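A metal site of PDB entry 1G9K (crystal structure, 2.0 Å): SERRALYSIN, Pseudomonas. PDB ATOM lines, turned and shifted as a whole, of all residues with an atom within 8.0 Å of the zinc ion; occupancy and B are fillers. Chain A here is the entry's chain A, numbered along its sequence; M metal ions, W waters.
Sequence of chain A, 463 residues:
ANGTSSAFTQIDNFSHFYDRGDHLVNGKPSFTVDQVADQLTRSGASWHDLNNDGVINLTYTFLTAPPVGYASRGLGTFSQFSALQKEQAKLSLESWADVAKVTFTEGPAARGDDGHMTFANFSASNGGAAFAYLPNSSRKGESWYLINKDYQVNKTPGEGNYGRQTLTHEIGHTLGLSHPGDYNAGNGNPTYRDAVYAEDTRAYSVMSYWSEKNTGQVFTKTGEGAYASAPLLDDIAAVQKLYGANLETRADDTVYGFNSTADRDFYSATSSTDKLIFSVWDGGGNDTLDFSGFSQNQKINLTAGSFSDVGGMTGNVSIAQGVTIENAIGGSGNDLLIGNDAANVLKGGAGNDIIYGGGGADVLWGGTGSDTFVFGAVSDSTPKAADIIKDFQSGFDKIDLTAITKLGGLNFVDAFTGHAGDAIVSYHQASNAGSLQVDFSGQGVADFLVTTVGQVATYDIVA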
ATOM      1  N   ALA A 130      24.744  -1.692   6.090  1.00  0.00           N
ATOM      2  CA  ALA A 130      23.371  -1.414   5.667  1.00  0.00           C
ATOM      3  C   ALA A 130      23.338  -1.410   4.151  1.00  0.00           C
ATOM      4  O   ALA A 130      24.369  -1.211   3.506  1.00  0.00           O
ATOM      5  CB  ALA A 130      22.939  -0.050   6.202  1.00  0.00           C
ATOM      6  N   PHE A 131      22.165  -1.639   3.566  1.00  0.00           N
ATOM      7  CA  PHE A 131      22.042  -1.602   2.114  1.00  0.00           C
ATOM      8  C   PHE A 131      20.601  -1.383   1.679  1.00  0.00           C
ATOM      9  O   PHE A 131      19.670  -1.562   2.457  1.00  0.00           O
ATOM     10  CB  PHE A 131      22.624  -2.874   1.475  1.00  0.00           C
ATOM     11  CG  PHE A 131      21.923  -4.133   1.879  1.00  0.00           C
ATOM     12  CD1 PHE A 131      20.821  -4.580   1.164  1.00  0.00           C
ATOM     13  CD2 PHE A 131      22.378  -4.873   2.970  1.00  0.00           C
ATOM     14  CE1 PHE A 131      20.174  -5.767   1.538  1.00  0.00           C
ATOM     15  CE2 PHE A 131      21.737  -6.052   3.347  1.00  0.00           C
ATOM     16  CZ  PHE A 131      20.635  -6.499   2.632  1.00  0.00           C
ATOM     17  N   ALA A 132      20.436  -0.992   0.418  1.00  0.00           N
ATOM     18  CA  ALA A 132      19.126  -0.718  -0.130  1.00  0.00           C
ATOM     19  C   ALA A 132      19.106  -1.073  -1.605  1.00  0.00           C
ATOM     20  O   ALA A 132      20.143  -1.342  -2.199  1.00  0.00           O
ATOM     21  CB  ALA A 132      18.786   0.747   0.047  1.00  0.00           C
ATOM     22  N   TYR A 162      26.335   9.076  12.633  1.00  0.00           N
ATOM     23  CA  TYR A 162      26.302   8.290  11.408  1.00  0.00           C
ATOM     24  C   TYR A 162      25.081   7.383  11.290  1.00  0.00           C
ATOM     25  O   TYR A 162      24.701   6.974  10.181  1.00  0.00           O
ATOM     26  CB  TYR A 162      27.586   7.473  11.249  1.00  0.00           C
ATOM     27  CG  TYR A 162      27.768   6.954   9.838  1.00  0.00           C
ATOM     28  CD1 TYR A 162      27.938   7.844   8.759  1.00  0.00           C
ATOM     29  CD2 TYR A 162      27.712   5.589   9.565  1.00  0.00           C
ATOM     30  CE1 TYR A 162      28.038   7.368   7.446  1.00  0.00           C
ATOM     31  CE2 TYR A 162      27.811   5.112   8.261  1.00  0.00           C
ATOM     32  CZ  TYR A 162      27.968   6.003   7.212  1.00  0.00           C
ATOM     33  OH  TYR A 162      28.050   5.521   5.926  1.00  0.00           O
ATOM     34  N   THR A 166      23.029   7.306   7.931  1.00  0.00           N
ATOM     35  CA  THR A 166      22.881   6.022   7.236  1.00  0.00           C
ATOM     36  C   THR A 166      21.437   5.881   6.758  1.00  0.00           C
ATOM     37  O   THR A 166      21.198   5.478   5.620  1.00  0.00           O
ATOM     38  CB  THR A 166      23.256   4.824   8.161  1.00  0.00           C
ATOM     39  OG1 THR A 166      24.674   4.834   8.386  1.00  0.00           O
ATOM     40  CG2 THR A 166      22.864   3.494   7.522  1.00  0.00           C
ATOM     41  N   HIS A 169      20.924   8.288   3.858  1.00  0.00           N
ATOM     42  CA  HIS A 169      21.717   7.784   2.742  1.00  0.00           C
ATOM     43  C   HIS A 169      21.041   6.588   2.062  1.00  0.00           C
ATOM     44  O   HIS A 169      20.897   6.556   0.841  1.00  0.00           O
ATOM     45  CB  HIS A 169      23.108   7.406   3.253  1.00  0.00           C
ATOM     46  CG  HIS A 169      23.995   6.738   2.246  1.00  0.00           C
ATOM     47  ND1 HIS A 169      25.114   7.345   1.729  1.00  0.00           N
ATOM     48  CD2 HIS A 169      23.972   5.484   1.710  1.00  0.00           C
ATOM     49  CE1 HIS A 169      25.752   6.505   0.928  1.00  0.00           C
ATOM     50  NE2 HIS A 169      25.074   5.362   0.906  1.00  0.00           N
ATOM     51  N   GLU A 170      20.620   5.602   2.858  1.00  0.00           N
ATOM     52  CA  GLU A 170      19.963   4.426   2.277  1.00  0.00           C
ATOM     53  C   GLU A 170      18.621   4.784   1.647  1.00  0.00           C
ATOM     54  O   GLU A 170      18.247   4.233   0.616  1.00  0.00           O
ATOM     55  CB  GLU A 170      19.767   3.330   3.336  1.00  0.00           C
ATOM     56  CG  GLU A 170      21.072   2.709   3.852  1.00  0.00           C
ATOM     57  CD  GLU A 170      22.020   2.287   2.733  1.00  0.00           C
ATOM     58  OE1 GLU A 170      21.547   1.819   1.681  1.00  0.00           O
ATOM     59  OE2 GLU A 170      23.249   2.416   2.908  1.00  0.00           O
ATOM     60  N   GLY A 172      18.048   7.503   0.284  1.00  0.00           N
ATOM     61  CA  GLY A 172      18.452   8.160  -0.954  1.00  0.00           C
ATOM     62  C   GLY A 172      18.565   7.134  -2.065  1.00  0.00           C
ATOM     63  O   GLY A 172      18.133   7.379  -3.199  1.00  0.00           O
ATOM     64  N   HIS A 173      19.159   5.988  -1.754  1.00  0.00           N
ATOM     65  CA  HIS A 173      19.288   4.904  -2.729  1.00  0.00           C
ATOM     66  C   HIS A 173      17.897   4.406  -3.161  1.00  0.00           C
ATOM     67  O   HIS A 173      17.668   4.207  -4.353  1.00  0.00           O
ATOM     68  CB  HIS A 173      20.070   3.710  -2.151  1.00  0.00           C
ATOM     69  CG  HIS A 173      21.556   3.914  -2.117  1.00  0.00           C
ATOM     70  ND1 HIS A 173      22.285   4.348  -3.200  1.00  0.00           N
ATOM     71  CD2 HIS A 173      22.460   3.638  -1.150  1.00  0.00           C
ATOM     72  CE1 HIS A 173      23.571   4.332  -2.907  1.00  0.00           C
ATOM     73  NE2 HIS A 173      23.703   3.905  -1.657  1.00  0.00           N
ATOM     74  N   LEU A 177      19.007   7.420  -6.107  1.00  0.00           N
ATOM     75  CA  LEU A 177      20.330   8.054  -6.125  1.00  0.00           C
ATOM     76  C   LEU A 177      21.454   7.044  -6.005  1.00  0.00           C
ATOM     77  O   LEU A 177      21.359   6.075  -5.237  1.00  0.00           O
ATOM     78  CB  LEU A 177      20.455   9.074  -4.977  1.00  0.00           C
ATOM     79  CG  LEU A 177      19.482  10.248  -4.993  1.00  0.00           C
ATOM     80  CD1 LEU A 177      19.864  11.223  -3.874  1.00  0.00           C
ATOM     81  CD2 LEU A 177      19.519  10.949  -6.321  1.00  0.00           C
ATOM     82  N   SER A 178      22.518   7.250  -6.767  1.00  0.00           N
ATOM     83  CA  SER A 178      23.686   6.379  -6.728  1.00  0.00           C
ATOM     84  C   SER A 178      24.784   7.089  -5.955  1.00  0.00           C
ATOM     85  O   SER A 178      24.617   8.223  -5.502  1.00  0.00           O
ATOM     86  CB  SER A 178      24.191   6.080  -8.141  1.00  0.00           C
ATOM     87  OG  SER A 178      23.185   5.488  -8.940  1.00  0.00           O
ATOM     88  N   HIS A 179      25.916   6.414  -5.774  1.00  0.00           N
ATOM     89  CA  HIS A 179      27.049   7.028  -5.106  1.00  0.00           C
ATOM     90  C   HIS A 179      27.623   7.960  -6.165  1.00  0.00           C
ATOM     91  O   HIS A 179      27.378   7.774  -7.357  1.00  0.00           O
ATOM     92  CB  HIS A 179      28.099   5.981  -4.747  1.00  0.00           C
ATOM     93  CG  HIS A 179      27.658   5.046  -3.668  1.00  0.00           C
ATOM     94  ND1 HIS A 179      27.960   3.700  -3.676  1.00  0.00           N
ATOM     95  CD2 HIS A 179      26.925   5.260  -2.553  1.00  0.00           C
ATOM     96  CE1 HIS A 179      27.430   3.129  -2.607  1.00  0.00           C
ATOM     97  NE2 HIS A 179      26.801   4.052  -1.914  1.00  0.00           N
ATOM     98  N   PRO A 180      28.367   8.981  -5.742  1.00  0.00           N
ATOM     99  CA  PRO A 180      28.970   9.944  -6.678  1.00  0.00           C
ATOM    100  C   PRO A 180      29.893   9.299  -7.727  1.00  0.00           C
ATOM    101  O   PRO A 180      30.211   9.906  -8.740  1.00  0.00           O
ATOM    102  CB  PRO A 180      29.721  10.894  -5.752  1.00  0.00           C
ATOM    103  CG  PRO A 180      28.872  10.891  -4.499  1.00  0.00           C
ATOM    104  CD  PRO A 180      28.571   9.418  -4.347  1.00  0.00           C
ATOM    105  N   TYR A 183      32.444   3.249  -6.915  1.00  0.00           N
ATOM    106  CA  TYR A 183      33.431   2.826  -5.941  1.00  0.00           C
ATOM    107  C   TYR A 183      33.732   1.332  -6.047  1.00  0.00           C
ATOM    108  O   TYR A 183      34.895   0.915  -6.021  1.00  0.00           O
ATOM    109  CB  TYR A 183      32.921   3.149  -4.545  1.00  0.00           C
ATOM    110  CG  TYR A 183      32.589   4.608  -4.326  1.00  0.00           C
ATOM    111  CD1 TYR A 183      31.689   4.981  -3.322  1.00  0.00           C
ATOM    112  CD2 TYR A 183      33.201   5.624  -5.066  1.00  0.00           C
ATOM    113  CE1 TYR A 183      31.404   6.313  -3.057  1.00  0.00           C
ATOM    114  CE2 TYR A 183      32.925   6.967  -4.819  1.00  0.00           C
ATOM    115  CZ  TYR A 183      32.031   7.302  -3.799  1.00  0.00           C
ATOM    116  OH  TYR A 183      31.753   8.612  -3.486  1.00  0.00           O
ATOM    117  N   VAL A 206      25.350  13.496   1.035  1.00  0.00           N
ATOM    118  CA  VAL A 206      25.364  12.438   2.030  1.00  0.00           C
ATOM    119  C   VAL A 206      25.577  11.087   1.339  1.00  0.00           C
ATOM    120  O   VAL A 206      25.714  10.062   2.010  1.00  0.00           O
ATOM    121  CB  VAL A 206      24.047  12.369   2.869  1.00  0.00           C
ATOM    122  CG1 VAL A 206      23.761  13.713   3.527  1.00  0.00           C
ATOM    123  CG2 VAL A 206      22.869  11.929   1.999  1.00  0.00           C
ATOM    124  N   MET A 207      25.600  11.062   0.012  1.00  0.00           N
ATOM    125  CA  MET A 207      25.802   9.803  -0.715  1.00  0.00           C
ATOM    126  C   MET A 207      27.276   9.476  -0.860  1.00  0.00           C
ATOM    127  O   MET A 207      27.630   8.369  -1.280  1.00  0.00           O
ATOM    128  CB  MET A 207      25.169   9.860  -2.121  1.00  0.00           C
ATOM    129  CG  MET A 207      23.701  10.195  -2.148  1.00  0.00           C
ATOM    130  SD  MET A 207      22.752   9.134  -1.048  1.00  0.00           S
ATOM    131  CE  MET A 207      22.856   7.563  -1.960  1.00  0.00           C
ATOM    132  N   SER A 208      28.145  10.426  -0.523  1.00  0.00           N
ATOM    133  CA  SER A 208      29.577  10.217  -0.653  1.00  0.00           C
ATOM    134  C   SER A 208      30.177   9.354   0.449  1.00  0.00           C
ATOM    135  O   SER A 208      29.692   9.364   1.577  1.00  0.00           O
ATOM    136  CB  SER A 208      30.310  11.568  -0.657  1.00  0.00           C
ATOM    137  OG  SER A 208      31.713  11.370  -0.697  1.00  0.00           O
ATOM    138  N   TYR A 209      31.230   8.611   0.112  1.00  0.00           N
ATOM    139  CA  TYR A 209      31.934   7.760   1.057  1.00  0.00           C
ATOM    140  C   TYR A 209      33.095   8.523   1.705  1.00  0.00           C
ATOM    141  O   TYR A 209      33.638   8.089   2.721  1.00  0.00           O
ATOM    142  CB  TYR A 209      32.543   6.547   0.330  1.00  0.00           C
ATOM    143  CG  TYR A 209      31.631   5.356   0.128  1.00  0.00           C
ATOM    144  CD1 TYR A 209      30.246   5.485   0.159  1.00  0.00           C
ATOM    145  CD2 TYR A 209      32.175   4.085  -0.106  1.00  0.00           C
ATOM    146  CE1 TYR A 209      29.418   4.372  -0.047  1.00  0.00           C
ATOM    147  CE2 TYR A 209      31.354   2.979  -0.309  1.00  0.00           C
ATOM    148  CZ  TYR A 209      29.976   3.130  -0.284  1.00  0.00           C
ATOM    149  OH  TYR A 209      29.169   2.025  -0.444  1.00  0.00           O
HETATM  150 ZN    ZN M   1      25.328   3.809  -0.483  1.00  0.00          ZN
HETATM  151  O   HOH W   1      25.336   1.971   0.701  1.00  0.00           O
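The zinc ion is bound by NE2 of His 173, NE2 of His 179, NE2 of His 169 and water W1.
Three residues have an atom within 4 Å of the zinc ion: His 169, His 173 and His 179. The nearest printed residue that does not touch the zinc ion is Tyr 209 (4.2 Å).
A ring nitrogen (ND1) of His 173 sits at hydrogen-bond distance from the backbone carbonyl oxygen (O) of Leu 177 (2.8 Å). The side-chain hydroxyl of Tyr 209 lies close to a ring nitrogen (NE2) of His 179. A ring nitrogen (ND1) of His 169 lies within hydrogen-bond range of the backbone carbonyl oxygen (O) of Val 206, 2.8 Å away.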
